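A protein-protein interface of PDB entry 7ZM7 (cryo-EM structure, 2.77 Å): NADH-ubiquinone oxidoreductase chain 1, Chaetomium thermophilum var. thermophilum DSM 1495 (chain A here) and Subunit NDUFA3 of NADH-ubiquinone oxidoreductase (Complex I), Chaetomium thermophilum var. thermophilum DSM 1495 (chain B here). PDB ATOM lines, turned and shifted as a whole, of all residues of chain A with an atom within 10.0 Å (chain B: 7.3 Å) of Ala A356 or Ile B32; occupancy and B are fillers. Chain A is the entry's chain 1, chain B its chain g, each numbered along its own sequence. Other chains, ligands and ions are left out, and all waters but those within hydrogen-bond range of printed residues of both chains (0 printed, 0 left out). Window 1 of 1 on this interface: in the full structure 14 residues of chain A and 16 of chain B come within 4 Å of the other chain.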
ATOM      1  N   SER A 157     -16.508 -20.445   6.190  1.00  0.00           N
ATOM      2  CA  SER A 157     -16.119 -19.304   6.997  1.00  0.00           C
ATOM      3  C   SER A 157     -15.052 -18.463   6.296  1.00  0.00           C
ATOM      4  O   SER A 157     -14.987 -17.245   6.489  1.00  0.00           O
ATOM      5  CB  SER A 157     -15.645 -19.794   8.364  1.00  0.00           C
ATOM      6  OG  SER A 157     -15.228 -18.736   9.186  1.00  0.00           O
ATOM      7  N   LEU A 161     -15.047 -14.287   4.004  1.00  0.00           N
ATOM      8  CA  LEU A 161     -14.119 -13.165   3.983  1.00  0.00           C
ATOM      9  C   LEU A 161     -13.956 -12.580   2.588  1.00  0.00           C
ATOM     10  O   LEU A 161     -13.630 -11.401   2.452  1.00  0.00           O
ATOM     11  CB  LEU A 161     -12.768 -13.603   4.546  1.00  0.00           C
ATOM     12  CG  LEU A 161     -12.749 -13.862   6.047  1.00  0.00           C
ATOM     13  CD1 LEU A 161     -11.670 -14.859   6.414  1.00  0.00           C
ATOM     14  CD2 LEU A 161     -12.587 -12.549   6.799  1.00  0.00           C
ATOM     15  N   MET A 164     -17.171 -10.322   1.891  1.00  0.00           N
ATOM     16  CA  MET A 164     -17.052  -8.982   2.525  1.00  0.00           C
ATOM     17  C   MET A 164     -16.360  -8.019   1.558  1.00  0.00           C
ATOM     18  O   MET A 164     -16.841  -6.884   1.428  1.00  0.00           O
ATOM     19  CB  MET A 164     -16.249  -9.085   3.823  1.00  0.00           C
ATOM     20  CG  MET A 164     -16.924  -9.942   4.874  1.00  0.00           C
ATOM     21  SD  MET A 164     -15.982 -10.044   6.410  1.00  0.00           S
ATOM     22  CE  MET A 164     -17.104 -11.002   7.427  1.00  0.00           C
ATOM     23  N   PRO A 189      -3.383 -14.986   3.952  1.00  0.00           N
ATOM     24  CA  PRO A 189      -3.535 -16.114   4.861  1.00  0.00           C
ATOM     25  C   PRO A 189      -4.896 -16.796   4.705  1.00  0.00           C
ATOM     26  O   PRO A 189      -4.976 -17.966   4.988  1.00  0.00           O
ATOM     27  CB  PRO A 189      -3.431 -15.465   6.247  1.00  0.00           C
ATOM     28  CG  PRO A 189      -3.879 -14.044   6.036  1.00  0.00           C
ATOM     29  CD  PRO A 189      -3.354 -13.699   4.662  1.00  0.00           C
ATOM     30  N   VAL A 190      -5.897 -16.070   4.198  1.00  0.00           N
ATOM     31  CA  VAL A 190      -7.196 -16.677   3.930  1.00  0.00           C
ATOM     32  C   VAL A 190      -7.107 -17.634   2.752  1.00  0.00           C
ATOM     33  O   VAL A 190      -7.790 -18.662   2.718  1.00  0.00           O
ATOM     34  CB  VAL A 190      -8.240 -15.577   3.682  1.00  0.00           C
ATOM     35  CG1 VAL A 190      -9.601 -16.165   3.502  1.00  0.00           C
ATOM     36  CG2 VAL A 190      -8.234 -14.591   4.813  1.00  0.00           C
ATOM     37  N   ILE A 193      -5.365 -20.964   3.905  1.00  0.00           N
ATOM     38  CA  ILE A 193      -6.303 -21.739   4.698  1.00  0.00           C
ATOM     39  C   ILE A 193      -7.349 -22.379   3.801  1.00  0.00           C
ATOM     40  O   ILE A 193      -7.727 -23.537   3.994  1.00  0.00           O
ATOM     41  CB  ILE A 193      -6.936 -20.838   5.773  1.00  0.00           C
ATOM     42  CG1 ILE A 193      -5.914 -20.521   6.847  1.00  0.00           C
ATOM     43  CG2 ILE A 193      -8.192 -21.479   6.362  1.00  0.00           C
ATOM     44  CD1 ILE A 193      -6.298 -19.368   7.683  1.00  0.00           C
ATOM     45  N   VAL A 349      -6.409 -24.606  15.518  1.00  0.00           N
ATOM     46  CA  VAL A 349      -5.497 -23.709  14.818  1.00  0.00           C
ATOM     47  C   VAL A 349      -6.246 -22.881  13.780  1.00  0.00           C
ATOM     48  O   VAL A 349      -6.324 -21.658  13.891  1.00  0.00           O
ATOM     49  CB  VAL A 349      -4.338 -24.481  14.156  1.00  0.00           C
ATOM     50  CG1 VAL A 349      -3.504 -23.548  13.305  1.00  0.00           C
ATOM     51  CG2 VAL A 349      -3.494 -25.167  15.190  1.00  0.00           C
ATOM     52  N   LEU A 350      -6.822 -23.544  12.778  1.00  0.00           N
ATOM     53  CA  LEU A 350      -7.344 -22.852  11.602  1.00  0.00           C
ATOM     54  C   LEU A 350      -8.558 -21.998  11.937  1.00  0.00           C
ATOM     55  O   LEU A 350      -8.575 -20.793  11.680  1.00  0.00           O
ATOM     56  CB  LEU A 350      -7.700 -23.869  10.519  1.00  0.00           C
ATOM     57  CG  LEU A 350      -6.592 -24.541   9.708  1.00  0.00           C
ATOM     58  CD1 LEU A 350      -7.214 -25.514   8.745  1.00  0.00           C
ATOM     59  CD2 LEU A 350      -5.791 -23.516   8.973  1.00  0.00           C
ATOM     60  N   LEU A 351      -9.596 -22.615  12.488  1.00  0.00           N
ATOM     61  CA  LEU A 351     -10.810 -21.878  12.831  1.00  0.00           C
ATOM     62  C   LEU A 351     -10.588 -20.745  13.818  1.00  0.00           C
ATOM     63  O   LEU A 351     -11.270 -19.718  13.685  1.00  0.00           O
ATOM     64  CB  LEU A 351     -11.868 -22.842  13.368  1.00  0.00           C
ATOM     65  CG  LEU A 351     -12.552 -23.731  12.344  1.00  0.00           C
ATOM     66  CD1 LEU A 351     -13.683 -24.439  13.014  1.00  0.00           C
ATOM     67  CD2 LEU A 351     -13.034 -22.925  11.161  1.00  0.00           C
ATOM     68  N   PRO A 352      -9.743 -20.869  14.844  1.00  0.00           N
ATOM     69  CA  PRO A 352      -9.443 -19.687  15.655  1.00  0.00           C
ATOM     70  C   PRO A 352      -8.864 -18.538  14.863  1.00  0.00           C
ATOM     71  O   PRO A 352      -9.258 -17.393  15.078  1.00  0.00           O
ATOM     72  CB  PRO A 352      -8.452 -20.236  16.687  1.00  0.00           C
ATOM     73  CG  PRO A 352      -8.854 -21.594  16.846  1.00  0.00           C
ATOM     74  CD  PRO A 352      -9.228 -22.080  15.494  1.00  0.00           C
ATOM     75  N   ILE A 353      -7.944 -18.816  13.944  1.00  0.00           N
ATOM     76  CA  ILE A 353      -7.382 -17.766  13.109  1.00  0.00           C
ATOM     77  C   ILE A 353      -8.456 -17.157  12.222  1.00  0.00           C
ATOM     78  O   ILE A 353      -8.510 -15.937  12.045  1.00  0.00           O
ATOM     79  CB  ILE A 353      -6.198 -18.307  12.284  1.00  0.00           C
ATOM     80  CG1 ILE A 353      -5.090 -18.831  13.190  1.00  0.00           C
ATOM     81  CG2 ILE A 353      -5.643 -17.237  11.382  1.00  0.00           C
ATOM     82  CD1 ILE A 353      -4.364 -17.756  13.979  1.00  0.00           C
ATOM     83  N   LEU A 354      -9.319 -17.991  11.641  1.00  0.00           N
ATOM     84  CA  LEU A 354     -10.374 -17.489  10.762  1.00  0.00           C
ATOM     85  C   LEU A 354     -11.348 -16.578  11.499  1.00  0.00           C
ATOM     86  O   LEU A 354     -11.752 -15.539  10.971  1.00  0.00           O
ATOM     87  CB  LEU A 354     -11.130 -18.653  10.135  1.00  0.00           C
ATOM     88  CG  LEU A 354     -10.518 -19.337   8.924  1.00  0.00           C
ATOM     89  CD1 LEU A 354     -11.357 -20.521   8.533  1.00  0.00           C
ATOM     90  CD2 LEU A 354     -10.401 -18.362   7.777  1.00  0.00           C
ATOM     91  N   PHE A 355     -11.757 -16.957  12.710  1.00  0.00           N
ATOM     92  CA  PHE A 355     -12.680 -16.122  13.467  1.00  0.00           C
ATOM     93  C   PHE A 355     -12.012 -14.850  13.945  1.00  0.00           C
ATOM     94  O   PHE A 355     -12.690 -13.848  14.189  1.00  0.00           O
ATOM     95  CB  PHE A 355     -13.240 -16.877  14.665  1.00  0.00           C
ATOM     96  CG  PHE A 355     -14.072 -18.055  14.302  1.00  0.00           C
ATOM     97  CD1 PHE A 355     -14.556 -18.213  13.013  1.00  0.00           C
ATOM     98  CD2 PHE A 355     -14.358 -19.016  15.240  1.00  0.00           C
ATOM     99  CE1 PHE A 355     -15.311 -19.307  12.665  1.00  0.00           C
ATOM    100  CE2 PHE A 355     -15.116 -20.117  14.906  1.00  0.00           C
ATOM    101  CZ  PHE A 355     -15.595 -20.264  13.612  1.00  0.00           C
ATOM    102  N   ALA A 356     -10.696 -14.883  14.122  1.00  0.00           N
ATOM    103  CA  ALA A 356      -9.948 -13.663  14.389  1.00  0.00           C
ATOM    104  C   ALA A 356      -9.955 -12.741  13.182  1.00  0.00           C
ATOM    105  O   ALA A 356     -10.028 -11.521  13.333  1.00  0.00           O
ATOM    106  CB  ALA A 356      -8.524 -14.019  14.789  1.00  0.00           C
ATOM    107  N   LEU A 357      -9.860 -13.305  11.975  1.00  0.00           N
ATOM    108  CA  LEU A 357      -9.876 -12.503  10.758  1.00  0.00           C
ATOM    109  C   LEU A 357     -11.280 -12.058  10.383  1.00  0.00           C
ATOM    110  O   LEU A 357     -11.438 -11.067   9.669  1.00  0.00           O
ATOM    111  CB  LEU A 357      -9.255 -13.285   9.607  1.00  0.00           C
ATOM    112  CG  LEU A 357      -7.732 -13.370   9.527  1.00  0.00           C
ATOM    113  CD1 LEU A 357      -7.345 -14.351   8.453  1.00  0.00           C
ATOM    114  CD2 LEU A 357      -7.097 -12.012   9.292  1.00  0.00           C
ATOM    115  N   ILE A 358     -12.300 -12.787  10.828  1.00  0.00           N
ATOM    116  CA  ILE A 358     -13.679 -12.358  10.622  1.00  0.00           C
ATOM    117  C   ILE A 358     -13.965 -11.091  11.399  1.00  0.00           C
ATOM    118  O   ILE A 358     -14.784 -10.269  10.984  1.00  0.00           O
ATOM    119  CB  ILE A 358     -14.660 -13.491  10.985  1.00  0.00           C
ATOM    120  CG1 ILE A 358     -14.575 -14.616   9.953  1.00  0.00           C
ATOM    121  CG2 ILE A 358     -16.076 -12.983  11.183  1.00  0.00           C
ATOM    122  CD1 ILE A 358     -15.330 -15.847  10.334  1.00  0.00           C
ATOM    123  N   VAL A 359     -13.320 -10.916  12.548  1.00  0.00           N
ATOM    124  CA  VAL A 359     -13.458  -9.656  13.270  1.00  0.00           C
ATOM    125  C   VAL A 359     -12.705  -8.553  12.552  1.00  0.00           C
ATOM    126  O   VAL A 359     -13.259  -7.491  12.259  1.00  0.00           O
ATOM    127  CB  VAL A 359     -12.969  -9.797  14.716  1.00  0.00           C
ATOM    128  CG1 VAL A 359     -12.669  -8.434  15.293  1.00  0.00           C
ATOM    129  CG2 VAL A 359     -13.988 -10.501  15.527  1.00  0.00           C
ATOM    130  N   LEU A 360     -11.449  -8.819  12.204  1.00  0.00           N
ATOM    131  CA  LEU A 360     -10.543  -7.767  11.763  1.00  0.00           C
ATOM    132  C   LEU A 360     -10.929  -7.200  10.397  1.00  0.00           C
ATOM    133  O   LEU A 360     -10.858  -5.987  10.188  1.00  0.00           O
ATOM    134  CB  LEU A 360      -9.118  -8.310  11.734  1.00  0.00           C
ATOM    135  CG  LEU A 360      -8.059  -7.389  11.134  1.00  0.00           C
ATOM    136  CD1 LEU A 360      -7.509  -6.416  12.152  1.00  0.00           C
ATOM    137  CD2 LEU A 360      -6.967  -8.197  10.501  1.00  0.00           C
ATOM    138  N   VAL A 361     -11.330  -8.046   9.453  1.00  0.00           N
ATOM    139  CA  VAL A 361     -11.512  -7.578   8.078  1.00  0.00           C
ATOM    140  C   VAL A 361     -12.603  -6.522   7.954  1.00  0.00           C
ATOM    141  O   VAL A 361     -12.305  -5.420   7.475  1.00  0.00           O
ATOM    142  CB  VAL A 361     -11.706  -8.777   7.131  1.00  0.00           C
ATOM    143  CG1 VAL A 361     -12.122  -8.330   5.766  1.00  0.00           C
ATOM    144  CG2 VAL A 361     -10.398  -9.506   7.008  1.00  0.00           C
ATOM    145  N   PRO A 362     -13.837  -6.745   8.409  1.00  0.00           N
ATOM    146  CA  PRO A 362     -14.821  -5.661   8.313  1.00  0.00           C
ATOM    147  C   PRO A 362     -14.449  -4.438   9.134  1.00  0.00           C
ATOM    148  O   PRO A 362     -14.901  -3.332   8.827  1.00  0.00           O
ATOM    149  CB  PRO A 362     -16.109  -6.324   8.814  1.00  0.00           C
ATOM    150  CG  PRO A 362     -15.677  -7.401   9.637  1.00  0.00           C
ATOM    151  CD  PRO A 362     -14.428  -7.929   9.050  1.00  0.00           C
ATOM    152  N   CYS A 363     -13.630  -4.604  10.163  1.00  0.00           N
ATOM    153  CA  CYS A 363     -13.190  -3.461  10.951  1.00  0.00           C
ATOM    154  C   CYS A 363     -12.272  -2.546  10.147  1.00  0.00           C
ATOM    155  O   CYS A 363     -12.343  -1.325  10.285  1.00  0.00           O
ATOM    156  CB  CYS A 363     -12.510  -3.952  12.225  1.00  0.00           C
ATOM    157  SG  CYS A 363     -13.641  -4.540  13.478  1.00  0.00           S
ATOM    158  N   ILE A 364     -11.404  -3.118   9.308  1.00  0.00           N
ATOM    159  CA  ILE A 364     -10.531  -2.318   8.448  1.00  0.00           C
ATOM    160  C   ILE A 364     -11.310  -1.707   7.289  1.00  0.00           C
ATOM    161  O   ILE A 364     -11.065  -0.563   6.897  1.00  0.00           O
ATOM    162  CB  ILE A 364      -9.357  -3.165   7.933  1.00  0.00           C
ATOM    163  CG1 ILE A 364      -8.642  -3.887   9.060  1.00  0.00           C
ATOM    164  CG2 ILE A 364      -8.354  -2.313   7.258  1.00  0.00           C
ATOM    165  CD1 ILE A 364      -7.682  -4.915   8.549  1.00  0.00           C
ATOM    166  N   ALA B  25      -0.766 -20.212  17.247  1.00  0.00           N
ATOM    167  CA  ALA B  25      -2.039 -20.007  16.562  1.00  0.00           C
ATOM    168  C   ALA B  25      -3.084 -19.446  17.508  1.00  0.00           C
ATOM    169  O   ALA B  25      -3.896 -18.600  17.122  1.00  0.00           O
ATOM    170  CB  ALA B  25      -2.538 -21.311  15.949  1.00  0.00           C
ATOM    171  N   PHE B  27      -2.376 -17.729  20.392  1.00  0.00           N
ATOM    172  CA  PHE B  27      -1.976 -16.418  20.881  1.00  0.00           C
ATOM    173  C   PHE B  27      -2.258 -15.344  19.847  1.00  0.00           C
ATOM    174  O   PHE B  27      -2.865 -14.312  20.150  1.00  0.00           O
ATOM    175  CB  PHE B  27      -0.498 -16.411  21.259  1.00  0.00           C
ATOM    176  CG  PHE B  27       0.025 -15.052  21.578  1.00  0.00           C
ATOM    177  CD1 PHE B  27      -0.199 -14.495  22.815  1.00  0.00           C
ATOM    178  CD2 PHE B  27       0.709 -14.314  20.629  1.00  0.00           C
ATOM    179  CE1 PHE B  27       0.255 -13.257  23.097  1.00  0.00           C
ATOM    180  CE2 PHE B  27       1.168 -13.077  20.910  1.00  0.00           C
ATOM    181  CZ  PHE B  27       0.942 -12.541  22.141  1.00  0.00           C
ATOM    182  N   PHE B  28      -1.840 -15.578  18.615  1.00  0.00           N
ATOM    183  CA  PHE B  28      -1.987 -14.584  17.572  1.00  0.00           C
ATOM    184  C   PHE B  28      -3.416 -14.478  17.060  1.00  0.00           C
ATOM    185  O   PHE B  28      -3.736 -13.510  16.371  1.00  0.00           O
ATOM    186  CB  PHE B  28      -0.997 -14.891  16.455  1.00  0.00           C
ATOM    187  CG  PHE B  28       0.430 -14.616  16.841  1.00  0.00           C
ATOM    188  CD1 PHE B  28       0.921 -13.331  16.844  1.00  0.00           C
ATOM    189  CD2 PHE B  28       1.268 -15.639  17.236  1.00  0.00           C
ATOM    190  CE1 PHE B  28       2.219 -13.081  17.210  1.00  0.00           C
ATOM    191  CE2 PHE B  28       2.559 -15.394  17.595  1.00  0.00           C
ATOM    192  CZ  PHE B  28       3.038 -14.118  17.585  1.00  0.00           C
ATOM    193  N   SER B  29      -4.285 -15.421  17.412  1.00  0.00           N
ATOM    194  CA  SER B  29      -5.712 -15.240  17.181  1.00  0.00           C
ATOM    195  C   SER B  29      -6.262 -14.116  18.042  1.00  0.00           C
ATOM    196  O   SER B  29      -7.014 -13.261  17.567  1.00  0.00           O
ATOM    197  CB  SER B  29      -6.456 -16.536  17.486  1.00  0.00           C
ATOM    198  OG  SER B  29      -6.066 -17.558  16.615  1.00  0.00           O
ATOM    199  N   VAL B  30      -5.909 -14.118  19.325  1.00  0.00           N
ATOM    200  CA  VAL B  30      -6.354 -13.076  20.238  1.00  0.00           C
ATOM    201  C   VAL B  30      -5.688 -11.758  19.903  1.00  0.00           C
ATOM    202  O   VAL B  30      -6.223 -10.686  20.196  1.00  0.00           O
ATOM    203  CB  VAL B  30      -6.075 -13.514  21.686  1.00  0.00           C
ATOM    204  CG1 VAL B  30      -6.684 -12.549  22.677  1.00  0.00           C
ATOM    205  CG2 VAL B  30      -6.608 -14.905  21.907  1.00  0.00           C
ATOM    206  N   VAL B  31      -4.510 -11.812  19.293  1.00  0.00           N
ATOM    207  CA  VAL B  31      -3.831 -10.600  18.866  1.00  0.00           C
ATOM    208  C   VAL B  31      -4.561  -9.968  17.696  1.00  0.00           C
ATOM    209  O   VAL B  31      -4.854  -8.768  17.700  1.00  0.00           O
ATOM    210  CB  VAL B  31      -2.369 -10.918  18.515  1.00  0.00           C
ATOM    211  CG1 VAL B  31      -1.661  -9.693  17.954  1.00  0.00           C
ATOM    212  CG2 VAL B  31      -1.671 -11.428  19.725  1.00  0.00           C
ATOM    213  N   ILE B  32      -4.851 -10.766  16.668  1.00  0.00           N
ATOM    214  CA  ILE B  32      -5.549 -10.254  15.494  1.00  0.00           C
ATOM    215  C   ILE B  32      -6.938  -9.768  15.869  1.00  0.00           C
ATOM    216  O   ILE B  32      -7.385  -8.711  15.411  1.00  0.00           O
ATOM    217  CB  ILE B  32      -5.613 -11.326  14.396  1.00  0.00           C
ATOM    218  CG1 ILE B  32      -4.217 -11.601  13.837  1.00  0.00           C
ATOM    219  CG2 ILE B  32      -6.548 -10.897  13.298  1.00  0.00           C
ATOM    220  CD1 ILE B  32      -4.081 -12.977  13.248  1.00  0.00           C
ATOM    221  N   GLY B  33      -7.638 -10.519  16.712  1.00  0.00           N
ATOM    222  CA  GLY B  33      -8.953 -10.083  17.133  1.00  0.00           C
ATOM    223  C   GLY B  33      -8.919  -8.747  17.844  1.00  0.00           C
ATOM    224  O   GLY B  33      -9.873  -7.969  17.769  1.00  0.00           O
ATOM    225  N   ALA B  34      -7.830  -8.470  18.563  1.00  0.00           N
ATOM    226  CA  ALA B  34      -7.688  -7.185  19.229  1.00  0.00           C
ATOM    227  C   ALA B  34      -7.315  -6.074  18.254  1.00  0.00           C
ATOM    228  O   ALA B  34      -7.606  -4.906  18.509  1.00  0.00           O
ATOM    229  CB  ALA B  34      -6.650  -7.294  20.334  1.00  0.00           C
ATOM    230  N   LEU B  35      -6.663  -6.413  17.143  1.00  0.00           N
ATOM    231  CA  LEU B  35      -6.281  -5.397  16.169  1.00  0.00           C
ATOM    232  C   LEU B  35      -7.490  -4.775  15.489  1.00  0.00           C
ATOM    233  O   LEU B  35      -7.428  -3.618  15.067  1.00  0.00           O
ATOM    234  CB  LEU B  35      -5.345  -5.996  15.132  1.00  0.00           C
ATOM    235  CG  LEU B  35      -3.997  -6.421  15.697  1.00  0.00           C
ATOM    236  CD1 LEU B  35      -3.177  -7.132  14.648  1.00  0.00           C
ATOM    237  CD2 LEU B  35      -3.273  -5.192  16.188  1.00  0.00           C
ATOM    238  N   GLY B  36      -8.576  -5.522  15.347  1.00  0.00           N
ATOM    239  CA  GLY B  36      -9.783  -4.984  14.782  1.00  0.00           C
ATOM    240  C   GLY B  36     -10.356  -3.894  15.648  1.00  0.00           C
ATOM    241  O   GLY B  36     -10.731  -2.819  15.181  1.00  0.00           O
ATOM    242  N   PRO B  37     -10.448  -4.164  16.947  1.00  0.00           N
ATOM    243  CA  PRO B  37     -10.892  -3.113  17.873  1.00  0.00           C
ATOM    244  C   PRO B  37      -9.974  -1.912  17.892  1.00  0.00           C
ATOM    245  O   PRO B  37     -10.458  -0.783  18.012  1.00  0.00           O
ATOM    246  CB  PRO B  37     -10.916  -3.832  19.222  1.00  0.00           C
ATOM    247  CG  PRO B  37     -11.281  -5.212  18.892  1.00  0.00           C
ATOM    248  N   VAL B  38      -8.662  -2.133  17.756  1.00  0.00           N
ATOM    249  CA  VAL B  38      -7.695  -1.043  17.668  1.00  0.00           C
ATOM    250  C   VAL B  38      -7.851  -0.277  16.364  1.00  0.00           C
ATOM    251  O   VAL B  38      -7.858   0.956  16.358  1.00  0.00           O
ATOM    252  CB  VAL B  38      -6.263  -1.585  17.808  1.00  0.00           C
ATOM    253  CG1 VAL B  38      -5.269  -0.473  17.603  1.00  0.00           C
ATOM    254  CG2 VAL B  38      -6.060  -2.196  19.163  1.00  0.00           C
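Printed residues of chain B within 4 Å of Val A349: Ala B25.
Of the printed residues of chain B, Pro A352 touches Ser B29.
Of the printed residues of chain B, Ile A353 touches Ala B25 (3.3 Å) and Ser B29 (3.1 Å).
Of the printed residues of chain B, Ala A356 touches Ser B29 (3.3 Å) and Ile B32 (3.5 Å).
Printed residues of chain B within 4 Å of Cys A363: Gly B36 (3.6 Å).
Ser B29 touches just these residues of chain A: Pro A352, Ile A353 and Ala A356.
Val B30 touches none of the printed residues of chain A.
Of chain A, only Ala A356 (3.5 Å) and Leu A360 (3.9 Å) come within 4 Å of Ile B32.
Gly B33 touches just one residue of chain A: Val A359 (3.8 Å).
Ala B34 touches none of the printed residues of chain A.
Of the printed residues of chain A, Gly B36 touches Leu A360 and Cys A363.
The nearest residue of chain B that does not touch Ala A356 is Gly B33 (4.1 Å).
The nearest residue of chain A that does not touch Ile B32 is Leu A357 (4.2 Å).
The nearest printed residue of chain A that does not touch Ala B25 is Pro A352 (4.9 Å).
The side-chain sulfur (SG) of Cys A363 sits at hydrogen-bond distance from the backbone carbonyl oxygen (O) of Val A359 (3.2 Å).
O of Ala B25 is in hydrogen-bond range of OG of Ser B29 (2.5 Å).
CG1 of Val A349 touches CB of Ala B25 (3.6 Å).
Pro A352 touches Ser B29.
Ala B25 touches Ile A353.
CB of Ala A356 touches O of Ser B29, 3.3 Å away.
O of Ala A356 touches CG2 of Ile B32, 3.5 Å away.
Val A359 touches Gly B33 (CG1 to O, 3.8 Å).
CG2 of Ile B32 touches CD2 of Leu A360, 3.9 Å away.
CB of Leu B35 touches CD1 of Leu A360, 3.7 Å away.
CD1 of Leu A360 touches N of Gly B36, 3.5 Å away.
N of Ile A353 lies close to OG of Ser B29, 3.5 Å away.
SG of Cys A363 sits close to O of Gly B36, at 3.8 Å.
Of the 13 printed residues of chain B, 6 touch a printed residue of chain A.
Of the 22 printed residues of chain A, 7 touch a printed residue of chain B.
Among the printed residues, no Asp or Glu carboxylate lies within 4 Å of a Lys or Arg side-chain nitrogen of the other chain.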
